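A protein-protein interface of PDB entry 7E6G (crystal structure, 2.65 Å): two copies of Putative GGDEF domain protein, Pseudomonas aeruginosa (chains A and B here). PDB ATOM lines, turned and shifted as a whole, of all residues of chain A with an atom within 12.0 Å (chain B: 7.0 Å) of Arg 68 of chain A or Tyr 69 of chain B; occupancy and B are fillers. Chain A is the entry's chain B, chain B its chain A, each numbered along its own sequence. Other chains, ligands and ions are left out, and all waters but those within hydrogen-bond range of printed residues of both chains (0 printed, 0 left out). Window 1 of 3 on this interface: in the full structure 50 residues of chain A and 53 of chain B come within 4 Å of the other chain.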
ATOM      1  N   MET A  57       2.967 -10.918  32.740  1.00  0.00           N
ATOM      2  CA  MET A  57       4.338 -10.428  32.833  1.00  0.00           C
ATOM      3  C   MET A  57       5.292 -11.266  31.988  1.00  0.00           C
ATOM      4  O   MET A  57       6.116 -10.728  31.240  1.00  0.00           O
ATOM      5  CB  MET A  57       4.781 -10.433  34.287  1.00  0.00           C
ATOM      6  CG  MET A  57       6.230 -10.096  34.476  1.00  0.00           C
ATOM      7  SD  MET A  57       6.665 -10.124  36.220  1.00  0.00           S
ATOM      8  CE  MET A  57       6.886 -11.880  36.472  1.00  0.00           C
ATOM      9  N   ALA A  58       5.214 -12.593  32.116  1.00  0.00           N
ATOM     10  CA  ALA A  58       6.108 -13.449  31.343  1.00  0.00           C
ATOM     11  C   ALA A  58       5.879 -13.275  29.842  1.00  0.00           C
ATOM     12  O   ALA A  58       6.836 -13.252  29.060  1.00  0.00           O
ATOM     13  CB  ALA A  58       5.933 -14.907  31.761  1.00  0.00           C
ATOM     14  N   ARG A  59       4.619 -13.144  29.423  1.00  0.00           N
ATOM     15  CA  ARG A  59       4.317 -12.947  28.007  1.00  0.00           C
ATOM     16  C   ARG A  59       4.967 -11.668  27.483  1.00  0.00           C
ATOM     17  O   ARG A  59       5.577 -11.650  26.402  1.00  0.00           O
ATOM     18  CB  ARG A  59       2.804 -12.910  27.816  1.00  0.00           C
ATOM     19  CG  ARG A  59       2.350 -13.051  26.394  1.00  0.00           C
ATOM     20  CD  ARG A  59       1.050 -12.306  26.165  1.00  0.00           C
ATOM     21  NE  ARG A  59       0.354 -12.800  24.986  1.00  0.00           N
ATOM     22  CZ  ARG A  59      -0.650 -12.171  24.377  1.00  0.00           C
ATOM     23  NH1 ARG A  59      -1.098 -11.006  24.837  1.00  0.00           N
ATOM     24  NH2 ARG A  59      -1.213 -12.722  23.307  1.00  0.00           N
ATOM     25  N   GLU A  60       4.869 -10.588  28.255  1.00  0.00           N
ATOM     26  CA  GLU A  60       5.465  -9.335  27.804  1.00  0.00           C
ATOM     27  C   GLU A  60       6.993  -9.413  27.825  1.00  0.00           C
ATOM     28  O   GLU A  60       7.665  -8.848  26.950  1.00  0.00           O
ATOM     29  CB  GLU A  60       4.935  -8.166  28.642  1.00  0.00           C
ATOM     30  CG  GLU A  60       4.613  -6.887  27.832  1.00  0.00           C
ATOM     31  CD  GLU A  60       3.812  -7.120  26.527  1.00  0.00           C
ATOM     32  OE1 GLU A  60       3.938  -6.274  25.608  1.00  0.00           O
ATOM     33  OE2 GLU A  60       3.038  -8.105  26.412  1.00  0.00           O
ATOM     34  N   GLN A  61       7.562 -10.145  28.782  1.00  0.00           N
ATOM     35  CA  GLN A  61       9.012 -10.282  28.812  1.00  0.00           C
ATOM     36  C   GLN A  61       9.514 -11.044  27.596  1.00  0.00           C
ATOM     37  O   GLN A  61      10.541 -10.689  27.006  1.00  0.00           O
ATOM     38  CB  GLN A  61       9.436 -10.960  30.105  1.00  0.00           C
ATOM     39  CG  GLN A  61       9.394 -10.002  31.269  1.00  0.00           C
ATOM     40  CD  GLN A  61       9.583 -10.691  32.589  1.00  0.00           C
ATOM     41  OE1 GLN A  61       9.724 -11.910  32.655  1.00  0.00           O
ATOM     42  NE2 GLN A  61       9.609  -9.912  33.656  1.00  0.00           N
ATOM     43  N   ASN A  62       8.783 -12.071  27.182  1.00  0.00           N
ATOM     44  CA  ASN A  62       9.194 -12.816  26.001  1.00  0.00           C
ATOM     45  C   ASN A  62       9.073 -11.970  24.735  1.00  0.00           C
ATOM     46  O   ASN A  62       9.951 -12.029  23.864  1.00  0.00           O
ATOM     47  CB  ASN A  62       8.375 -14.090  25.869  1.00  0.00           C
ATOM     48  CG  ASN A  62       8.840 -14.943  24.724  1.00  0.00           C
ATOM     49  OD1 ASN A  62       9.827 -15.672  24.852  1.00  0.00           O
ATOM     50  ND2 ASN A  62       8.154 -14.846  23.582  1.00  0.00           N
ATOM     51  N   LEU A  63       7.990 -11.186  24.604  1.00  0.00           N
ATOM     52  CA  LEU A  63       7.861 -10.297  23.445  1.00  0.00           C
ATOM     53  C   LEU A  63       8.990  -9.264  23.400  1.00  0.00           C
ATOM     54  O   LEU A  63       9.517  -8.943  22.321  1.00  0.00           O
ATOM     55  CB  LEU A  63       6.496  -9.604  23.459  1.00  0.00           C
ATOM     56  CG  LEU A  63       5.282 -10.493  23.160  1.00  0.00           C
ATOM     57  CD1 LEU A  63       4.024  -9.671  22.947  1.00  0.00           C
ATOM     58  CD2 LEU A  63       5.534 -11.378  21.956  1.00  0.00           C
ATOM     59  N   SER A  64       9.389  -8.751  24.566  1.00  0.00           N
ATOM     60  CA  SER A  64      10.501  -7.807  24.626  1.00  0.00           C
ATOM     61  C   SER A  64      11.822  -8.470  24.232  1.00  0.00           C
ATOM     62  O   SER A  64      12.628  -7.884  23.496  1.00  0.00           O
ATOM     63  CB  SER A  64      10.578  -7.202  26.028  1.00  0.00           C
ATOM     64  OG  SER A  64      11.915  -6.930  26.407  1.00  0.00           O
ATOM     65  N   LEU A  65      12.062  -9.696  24.708  1.00  0.00           N
ATOM     66  CA  LEU A  65      13.265 -10.417  24.309  1.00  0.00           C
ATOM     67  C   LEU A  65      13.267 -10.710  22.815  1.00  0.00           C
ATOM     68  O   LEU A  65      14.325 -10.699  22.181  1.00  0.00           O
ATOM     69  CB  LEU A  65      13.381 -11.713  25.106  1.00  0.00           C
ATOM     70  CG  LEU A  65      14.639 -12.553  24.872  1.00  0.00           C
ATOM     71  CD1 LEU A  65      15.880 -11.818  25.352  1.00  0.00           C
ATOM     72  CD2 LEU A  65      14.508 -13.897  25.566  1.00  0.00           C
ATOM     73  N   SER A  66      12.094 -10.949  22.228  1.00  0.00           N
ATOM     74  CA  SER A  66      12.000 -11.168  20.784  1.00  0.00           C
ATOM     75  C   SER A  66      12.407  -9.916  20.004  1.00  0.00           C
ATOM     76  O   SER A  66      13.218  -9.975  19.059  1.00  0.00           O
ATOM     77  CB  SER A  66      10.572 -11.592  20.436  1.00  0.00           C
ATOM     78  OG  SER A  66      10.405 -11.755  19.044  1.00  0.00           O
ATOM     79  N   GLU A  67      11.842  -8.770  20.389  1.00  0.00           N
ATOM     80  CA  GLU A  67      12.237  -7.509  19.770  1.00  0.00           C
ATOM     81  C   GLU A  67      13.741  -7.272  19.911  1.00  0.00           C
ATOM     82  O   GLU A  67      14.412  -6.873  18.947  1.00  0.00           O
ATOM     83  CB  GLU A  67      11.449  -6.359  20.393  1.00  0.00           C
ATOM     84  CG  GLU A  67      10.710  -5.482  19.389  1.00  0.00           C
ATOM     85  CD  GLU A  67      10.008  -4.304  20.062  1.00  0.00           C
ATOM     86  OE1 GLU A  67       9.771  -4.362  21.301  1.00  0.00           O
ATOM     87  OE2 GLU A  67       9.701  -3.317  19.348  1.00  0.00           O
ATOM     88  N   ARG A  68      14.279  -7.497  21.118  1.00  0.00           N
ATOM     89  CA  ARG A  68      15.712  -7.337  21.338  1.00  0.00           C
ATOM     90  C   ARG A  68      16.519  -8.240  20.416  1.00  0.00           C
ATOM     91  O   ARG A  68      17.569  -7.836  19.899  1.00  0.00           O
ATOM     92  CB  ARG A  68      16.055  -7.628  22.793  1.00  0.00           C
ATOM     93  CG  ARG A  68      16.900  -6.561  23.425  1.00  0.00           C
ATOM     94  CD  ARG A  68      16.533  -6.319  24.882  1.00  0.00           C
ATOM     95  NE  ARG A  68      16.898  -7.441  25.741  1.00  0.00           N
ATOM     96  CZ  ARG A  68      16.066  -8.032  26.601  1.00  0.00           C
ATOM     97  NH1 ARG A  68      14.812  -7.605  26.720  1.00  0.00           N
ATOM     98  NH2 ARG A  68      16.492  -9.057  27.339  1.00  0.00           N
ATOM     99  N   TYR A  69      16.039  -9.463  20.189  1.00  0.00           N
ATOM    100  CA  TYR A  69      16.779 -10.404  19.358  1.00  0.00           C
ATOM    101  C   TYR A  69      16.869  -9.915  17.915  1.00  0.00           C
ATOM    102  O   TYR A  69      17.938  -9.976  17.282  1.00  0.00           O
ATOM    103  CB  TYR A  69      16.115 -11.780  19.443  1.00  0.00           C
ATOM    104  CG  TYR A  69      16.676 -12.784  18.484  1.00  0.00           C
ATOM    105  CD1 TYR A  69      17.892 -13.397  18.731  1.00  0.00           C
ATOM    106  CD2 TYR A  69      15.995 -13.116  17.318  1.00  0.00           C
ATOM    107  CE1 TYR A  69      18.415 -14.314  17.855  1.00  0.00           C
ATOM    108  CE2 TYR A  69      16.516 -14.035  16.430  1.00  0.00           C
ATOM    109  CZ  TYR A  69      17.728 -14.630  16.709  1.00  0.00           C
ATOM    110  OH  TYR A  69      18.272 -15.546  15.838  1.00  0.00           O
ATOM    111  N   HIS A  70      15.768  -9.394  17.381  1.00  0.00           N
ATOM    112  CA  HIS A  70      15.828  -8.949  15.986  1.00  0.00           C
ATOM    113  C   HIS A  70      16.624  -7.645  15.844  1.00  0.00           C
ATOM    114  O   HIS A  70      17.374  -7.458  14.863  1.00  0.00           O
ATOM    115  CB  HIS A  70      14.417  -8.843  15.416  1.00  0.00           C
ATOM    116  CG  HIS A  70      13.750 -10.177  15.270  1.00  0.00           C
ATOM    117  ND1 HIS A  70      12.968 -10.730  16.264  1.00  0.00           N
ATOM    118  CD2 HIS A  70      13.790 -11.093  14.270  1.00  0.00           C
ATOM    119  CE1 HIS A  70      12.538 -11.919  15.875  1.00  0.00           C
ATOM    120  NE2 HIS A  70      13.025 -12.163  14.670  1.00  0.00           N
ATOM    121  N   LYS A  71      16.516  -6.751  16.830  1.00  0.00           N
ATOM    122  CA  LYS A  71      17.391  -5.587  16.830  1.00  0.00           C
ATOM    123  C   LYS A  71      18.867  -5.992  16.942  1.00  0.00           C
ATOM    124  O   LYS A  71      19.734  -5.313  16.374  1.00  0.00           O
ATOM    125  CB  LYS A  71      16.983  -4.621  17.946  1.00  0.00           C
ATOM    126  CG  LYS A  71      15.510  -4.194  17.870  1.00  0.00           C
ATOM    127  CD  LYS A  71      15.199  -2.919  18.685  1.00  0.00           C
ATOM    128  CE  LYS A  71      14.015  -3.131  19.645  1.00  0.00           C
ATOM    129  NZ  LYS A  71      14.411  -3.485  21.062  1.00  0.00           N
ATOM    130  N   GLN A  72      19.175  -7.103  17.630  1.00  0.00           N
ATOM    131  CA  GLN A  72      20.555  -7.591  17.655  1.00  0.00           C
ATOM    132  C   GLN A  72      21.017  -8.009  16.264  1.00  0.00           C
ATOM    133  O   GLN A  72      22.161  -7.722  15.865  1.00  0.00           O
ATOM    134  CB  GLN A  72      20.699  -8.765  18.628  1.00  0.00           C
ATOM    135  CG  GLN A  72      21.222  -8.380  20.006  1.00  0.00           C
ATOM    136  CD  GLN A  72      22.486  -7.543  19.962  1.00  0.00           C
ATOM    137  OE1 GLN A  72      22.468  -6.349  20.274  1.00  0.00           O
ATOM    138  NE2 GLN A  72      23.604  -8.176  19.621  1.00  0.00           N
ATOM    139  N   LEU A  73      20.151  -8.709  15.521  1.00  0.00           N
ATOM    140  CA  LEU A  73      20.518  -9.105  14.158  1.00  0.00           C
ATOM    141  C   LEU A  73      20.887  -7.886  13.313  1.00  0.00           C
ATOM    142  O   LEU A  73      21.968  -7.821  12.695  1.00  0.00           O
ATOM    143  CB  LEU A  73      19.374  -9.881  13.509  1.00  0.00           C
ATOM    144  CG  LEU A  73      19.319 -11.415  13.621  1.00  0.00           C
ATOM    145  CD1 LEU A  73      19.747 -11.914  14.990  1.00  0.00           C
ATOM    146  CD2 LEU A  73      17.900 -11.920  13.273  1.00  0.00           C
ATOM    147  N   ARG A  74      20.003  -6.889  13.304  1.00  0.00           N
ATOM    148  CA  ARG A  74      20.284  -5.686  12.523  1.00  0.00           C
ATOM    149  C   ARG A  74      21.515  -4.942  13.044  1.00  0.00           C
ATOM    150  O   ARG A  74      22.248  -4.336  12.254  1.00  0.00           O
ATOM    151  CB  ARG A  74      19.069  -4.756  12.496  1.00  0.00           C
ATOM    152  CG  ARG A  74      17.718  -5.436  12.255  1.00  0.00           C
ATOM    153  CD  ARG A  74      17.722  -6.352  11.027  1.00  0.00           C
ATOM    154  NE  ARG A  74      16.972  -7.590  11.276  1.00  0.00           N
ATOM    155  CZ  ARG A  74      17.010  -8.664  10.488  1.00  0.00           C
ATOM    156  NH1 ARG A  74      16.298  -9.748  10.795  1.00  0.00           N
ATOM    157  NH2 ARG A  74      17.761  -8.653   9.395  1.00  0.00           N
ATOM    158  N   ARG A  75      21.781  -4.977  14.352  1.00  0.00           N
ATOM    159  CA  ARG A  75      22.944  -4.255  14.864  1.00  0.00           C
ATOM    160  C   ARG A  75      24.235  -4.894  14.389  1.00  0.00           C
ATOM    161  O   ARG A  75      25.203  -4.192  14.084  1.00  0.00           O
ATOM    162  CB  ARG A  75      22.921  -4.199  16.392  1.00  0.00           C
ATOM    163  CG  ARG A  75      24.160  -3.616  17.030  1.00  0.00           C
ATOM    164  CD  ARG A  75      24.375  -2.119  16.653  1.00  0.00           C
ATOM    165  NE  ARG A  75      23.222  -1.246  16.930  1.00  0.00           N
ATOM    166  CZ  ARG A  75      22.925  -0.737  18.124  1.00  0.00           C
ATOM    167  NH1 ARG A  75      23.672  -1.009  19.187  1.00  0.00           N
ATOM    168  NH2 ARG A  75      21.867   0.042  18.259  1.00  0.00           N
ATOM    169  N   LEU A  76      24.285  -6.228  14.348  1.00  0.00           N
ATOM    170  CA  LEU A  76      25.473  -6.869  13.795  1.00  0.00           C
ATOM    171  C   LEU A  76      25.675  -6.467  12.336  1.00  0.00           C
ATOM    172  O   LEU A  76      26.808  -6.178  11.910  1.00  0.00           O
ATOM    173  CB  LEU A  76      25.382  -8.388  13.937  1.00  0.00           C
ATOM    174  CG  LEU A  76      26.492  -9.152  13.189  1.00  0.00           C
ATOM    175  CD1 LEU A  76      27.905  -8.705  13.571  1.00  0.00           C
ATOM    176  CD2 LEU A  76      26.345 -10.669  13.347  1.00  0.00           C
ATOM    177  N   GLU A  77      24.584  -6.394  11.559  1.00  0.00           N
ATOM    178  CA  GLU A  77      24.777  -5.979  10.165  1.00  0.00           C
ATOM    179  C   GLU A  77      25.265  -4.527  10.056  1.00  0.00           C
ATOM    180  O   GLU A  77      26.133  -4.223   9.225  1.00  0.00           O
ATOM    181  CB  GLU A  77      23.510  -6.206   9.352  1.00  0.00           C
ATOM    182  CG  GLU A  77      23.599  -7.477   8.532  1.00  0.00           C
ATOM    183  CD  GLU A  77      22.321  -8.289   8.568  1.00  0.00           C
ATOM    184  OE1 GLU A  77      22.398  -9.535   8.383  1.00  0.00           O
ATOM    185  OE2 GLU A  77      21.243  -7.675   8.781  1.00  0.00           O
ATOM    186  N   SER B  64      14.607 -21.041  25.220  1.00  0.00           N
ATOM    187  CA  SER B  64      15.160 -21.231  23.882  1.00  0.00           C
ATOM    188  C   SER B  64      15.506 -19.888  23.222  1.00  0.00           C
ATOM    189  O   SER B  64      16.604 -19.707  22.660  1.00  0.00           O
ATOM    190  CB  SER B  64      14.156 -22.023  23.044  1.00  0.00           C
ATOM    191  OG  SER B  64      14.621 -22.243  21.728  1.00  0.00           O
ATOM    192  N   LEU B  65      14.571 -18.928  23.287  1.00  0.00           N
ATOM    193  CA  LEU B  65      14.819 -17.607  22.704  1.00  0.00           C
ATOM    194  C   LEU B  65      15.999 -16.908  23.374  1.00  0.00           C
ATOM    195  O   LEU B  65      16.786 -16.214  22.711  1.00  0.00           O
ATOM    196  CB  LEU B  65      13.567 -16.739  22.812  1.00  0.00           C
ATOM    197  CG  LEU B  65      13.650 -15.371  22.115  1.00  0.00           C
ATOM    198  CD1 LEU B  65      14.051 -15.535  20.652  1.00  0.00           C
ATOM    199  CD2 LEU B  65      12.336 -14.579  22.236  1.00  0.00           C
ATOM    200  N   SER B  66      16.129 -17.074  24.694  1.00  0.00           N
ATOM    201  CA  SER B  66      17.225 -16.462  25.433  1.00  0.00           C
ATOM    202  C   SER B  66      18.572 -17.061  25.042  1.00  0.00           C
ATOM    203  O   SER B  66      19.573 -16.339  24.926  1.00  0.00           O
ATOM    204  CB  SER B  66      16.978 -16.630  26.923  1.00  0.00           C
ATOM    205  OG  SER B  66      17.882 -15.841  27.675  1.00  0.00           O
ATOM    206  N   GLU B  67      18.638 -18.283  24.783  1.00  0.00           N
ATOM    207  CA  GLU B  67      19.804 -18.873  24.324  1.00  0.00           C
ATOM    208  C   GLU B  67      20.174 -18.382  22.969  1.00  0.00           C
ATOM    209  O   GLU B  67      21.239 -18.221  22.638  1.00  0.00           O
ATOM    210  CB  GLU B  67      19.502 -20.335  24.283  1.00  0.00           C
ATOM    211  CG  GLU B  67      20.353 -21.247  25.073  1.00  0.00           C
ATOM    212  CD  GLU B  67      19.806 -22.650  25.099  1.00  0.00           C
ATOM    213  OE1 GLU B  67      18.608 -22.844  25.157  1.00  0.00           O
ATOM    214  OE2 GLU B  67      20.602 -23.584  25.133  1.00  0.00           O
ATOM    215  N   ARG B  68      19.266 -18.061  22.151  1.00  0.00           N
ATOM    216  CA  ARG B  68      19.627 -17.503  20.927  1.00  0.00           C
ATOM    217  C   ARG B  68      20.155 -16.190  20.985  1.00  0.00           C
ATOM    218  O   ARG B  68      20.824 -15.876  20.224  1.00  0.00           O
ATOM    219  CB  ARG B  68      18.530 -17.544  19.957  1.00  0.00           C
ATOM    220  CG  ARG B  68      17.966 -18.885  19.887  1.00  0.00           C
ATOM    221  CD  ARG B  68      17.398 -19.293  18.566  1.00  0.00           C
ATOM    222  NE  ARG B  68      15.990 -18.997  18.448  1.00  0.00           N
ATOM    223  CZ  ARG B  68      15.435 -18.691  17.306  1.00  0.00           C
ATOM    224  NH1 ARG B  68      16.188 -18.686  16.236  1.00  0.00           N
ATOM    225  NH2 ARG B  68      14.168 -18.387  17.251  1.00  0.00           N
ATOM    226  N   TYR B  69      19.664 -15.390  21.834  1.00  0.00           N
ATOM    227  CA  TYR B  69      20.053 -14.098  22.067  1.00  0.00           C
ATOM    228  C   TYR B  69      21.438 -14.003  22.542  1.00  0.00           C
ATOM    229  O   TYR B  69      22.093 -13.162  22.196  1.00  0.00           O
ATOM    230  CB  TYR B  69      19.087 -13.522  23.041  1.00  0.00           C
ATOM    231  CG  TYR B  69      19.351 -12.168  23.372  1.00  0.00           C
ATOM    232  CD1 TYR B  69      19.141 -11.211  22.471  1.00  0.00           C
ATOM    233  CD2 TYR B  69      19.917 -11.834  24.538  1.00  0.00           C
ATOM    234  CE1 TYR B  69      19.454  -9.925  22.736  1.00  0.00           C
ATOM    235  CE2 TYR B  69      20.233 -10.568  24.811  1.00  0.00           C
ATOM    236  CZ  TYR B  69      19.989  -9.622  23.907  1.00  0.00           C
ATOM    237  OH  TYR B  69      20.277  -8.376  24.174  1.00  0.00           O
ATOM    238  N   HIS B  70      21.836 -14.836  23.404  1.00  0.00           N
ATOM    239  CA  HIS B  70      23.117 -14.941  23.900  1.00  0.00           C
ATOM    240  C   HIS B  70      24.097 -15.397  22.875  1.00  0.00           C
ATOM    241  O   HIS B  70      25.134 -15.006  22.902  1.00  0.00           O
ATOM    242  CB  HIS B  70      23.077 -15.679  25.206  1.00  0.00           C
ATOM    243  CG  HIS B  70      22.605 -14.853  26.343  1.00  0.00           C
ATOM    244  ND1 HIS B  70      21.325 -14.862  26.790  1.00  0.00           N
ATOM    245  CD2 HIS B  70      23.243 -13.955  27.086  1.00  0.00           C
ATOM    246  CE1 HIS B  70      21.193 -14.005  27.750  1.00  0.00           C
ATOM    247  NE2 HIS B  70      22.346 -13.440  27.950  1.00  0.00           N
ATOM    248  N   LYS B  71      23.738 -16.264  21.979  1.00  0.00           N
ATOM    249  CA  LYS B  71      24.566 -16.687  20.906  1.00  0.00           C
ATOM    250  C   LYS B  71      24.873 -15.587  19.995  1.00  0.00           C
ATOM    251  O   LYS B  71      25.894 -15.480  19.599  1.00  0.00           O
ATOM    252  CB  LYS B  71      23.932 -17.771  20.178  1.00  0.00           C
ATOM    253  CG  LYS B  71      24.088 -19.036  20.853  1.00  0.00           C
ATOM    254  CD  LYS B  71      23.609 -20.142  19.998  1.00  0.00           C
ATOM    255  CE  LYS B  71      23.761 -21.488  20.654  1.00  0.00           C
ATOM    256  NZ  LYS B  71      22.478 -22.139  21.003  1.00  0.00           N
ATOM    257  N   GLN B  72      23.943 -14.754  19.706  1.00  0.00           N
ATOM    258  CA  GLN B  72      24.056 -13.644  18.928  1.00  0.00           C
ATOM    259  C   GLN B  72      24.964 -12.683  19.509  1.00  0.00           C
ATOM    260  O   GLN B  72      25.655 -12.122  18.837  1.00  0.00           O
ATOM    261  CB  GLN B  72      22.770 -13.039  18.912  1.00  0.00           C
ATOM    262  CG  GLN B  72      21.997 -13.171  17.706  1.00  0.00           C
ATOM    263  CD  GLN B  72      22.668 -13.867  16.599  1.00  0.00           C
ATOM    264  OE1 GLN B  72      22.393 -15.025  16.347  1.00  0.00           O
ATOM    265  NE2 GLN B  72      23.454 -13.153  15.853  1.00  0.00           N
ATOM    266  N   LEU B  73      24.950 -12.467  20.790  1.00  0.00           N
ATOM    267  CA  LEU B  73      25.828 -11.610  21.441  1.00  0.00           C
ATOM    268  C   LEU B  73      27.222 -11.961  21.377  1.00  0.00           C
ATOM    269  O   LEU B  73      27.996 -11.203  21.413  1.00  0.00           O
ATOM    270  CB  LEU B  73      25.395 -11.450  22.826  1.00  0.00           C
ATOM    271  CG  LEU B  73      24.684 -10.298  23.440  1.00  0.00           C
ATOM    272  CD1 LEU B  73      23.497  -9.876  22.686  1.00  0.00           C
ATOM    273  CD2 LEU B  73      24.184 -10.949  24.624  1.00  0.00           C
ATOM    274  N   ARG B  74      27.483 -13.183  21.463  1.00  0.00           N
ATOM    275  CA  ARG B  74      28.728 -13.741  21.319  1.00  0.00           C
ATOM    276  C   ARG B  74      29.260 -13.642  20.026  1.00  0.00           C
ATOM    277  O   ARG B  74      30.309 -13.412  19.895  1.00  0.00           O
ATOM    278  CB  ARG B  74      28.626 -15.130  21.712  1.00  0.00           C
ATOM    279  CG  ARG B  74      28.461 -15.190  23.128  1.00  0.00           C
ATOM    280  CD  ARG B  74      28.788 -16.536  23.583  1.00  0.00           C
ATOM    281  NE  ARG B  74      27.794 -17.541  23.322  1.00  0.00           N
ATOM    282  CZ  ARG B  74      26.851 -17.916  24.160  1.00  0.00           C
ATOM    283  NH1 ARG B  74      26.035 -18.842  23.800  1.00  0.00           N
ATOM    284  NH2 ARG B  74      26.707 -17.342  25.323  1.00  0.00           N
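Of chain B, only Tyr 69 (3.8 Å) comes within 4 Å of Arg 68 of chain A. Printed residues of chain A within 4 Å of Tyr 69 of chain B: Arg 68 (3.8 Å), Tyr 69 (3.99 Å) and Gln 72 (3.6 Å). Ser 66 of chain B touches just one residue of chain A: Leu 65. No residue of chain A comes within 4 Å of His 70 of chain B. Lys 71 of chain B touches none of the printed residues of chain A. Of chain A, only Tyr 69 (3.8 Å) and Leu 73 (3.7 Å) come within 4 Å of Gln 72 of chain B. Printed residues of chain A within 4 Å of Leu 73 of chain B: Gln 72. Printed residues of chain B within 4 Å of Leu 73 of chain A: Gln 72. Of the printed residues of chain B, Leu 65 of chain A touches Leu 65 and Ser 66. Of the printed residues of chain B, Gln 72 of chain A touches Tyr 69 and Leu 73. Of the printed residues of chain B, Asn 62 of chain A touches Leu 65 (3.8 Å). The nearest printed residue of chain B that does not touch Leu 65 of chain A is Tyr 69 of chain B (4.01 Å).
Leu 65 of chain B touches Asn 62 of chain A (CD2 to OD1, 3.8 Å). Leu 65 of chain A touches Leu 65 of chain B. CD2 of Leu 65 of chain A touches N of Ser 66 of chain B (3.7 Å). CD2 of Leu 65 of chain B touches N of Ser 66 of chain A (3.6 Å). Tyr 69 of chain B touches Arg 68 of chain A (OH to NE, 3.8 Å). Tyr 69 of chain B touches Tyr 69 of chain A (CD1 to CA, 3.99 Å). Tyr 69 of chain A touches Gln 72 of chain B. CG of Gln 72 of chain A touches CE1 of Tyr 69 of chain B, at 3.6 Å. Leu 73 of chain B touches Gln 72 of chain A. CD1 of Leu 73 of chain A touches CG of Gln 72 of chain B, at 3.7 Å.
ND1 of His 70 of chain B sits at hydrogen-bond distance from O of Ser 66 of chain B (3.0 Å). The guanidinium group of Arg 68 of chain A is in hydrogen-bond range of the side-chain hydroxyl of Ser 64 of chain A (3.0 Å). A ring nitrogen (ND1) of His 70 of chain A is in hydrogen-bond range of the backbone carbonyl oxygen (O) of Ser 66 of chain A.
Leu 65 of chain B touches its own counterpart, Leu 65 of chain A. Leu 65 of chain A touches Ser 66 of chain B, and with the chains exchanged Ser 66 of chain A touches Leu 65 of chain B. Arg 68 of chain A touches Tyr 69 of chain B, and with the chains exchanged Tyr 69 of chain A touches Arg 68 of chain B. Tyr 69 of chain A touches its own counterpart, Tyr 69 of chain B. 11 positions are printed for both chains. Of the 11 pairs that touch across the chains among the printed residues, 10 have their exchanged pair printed and touching as well.
Along chain B the printed residues that touch a printed residue of chain A span positions 65 to 73. Of the 21 printed residues of chain A, 7 touch a printed residue of chain B. Along chain A the printed residues that touch a printed residue of chain B span positions 62 to 73.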
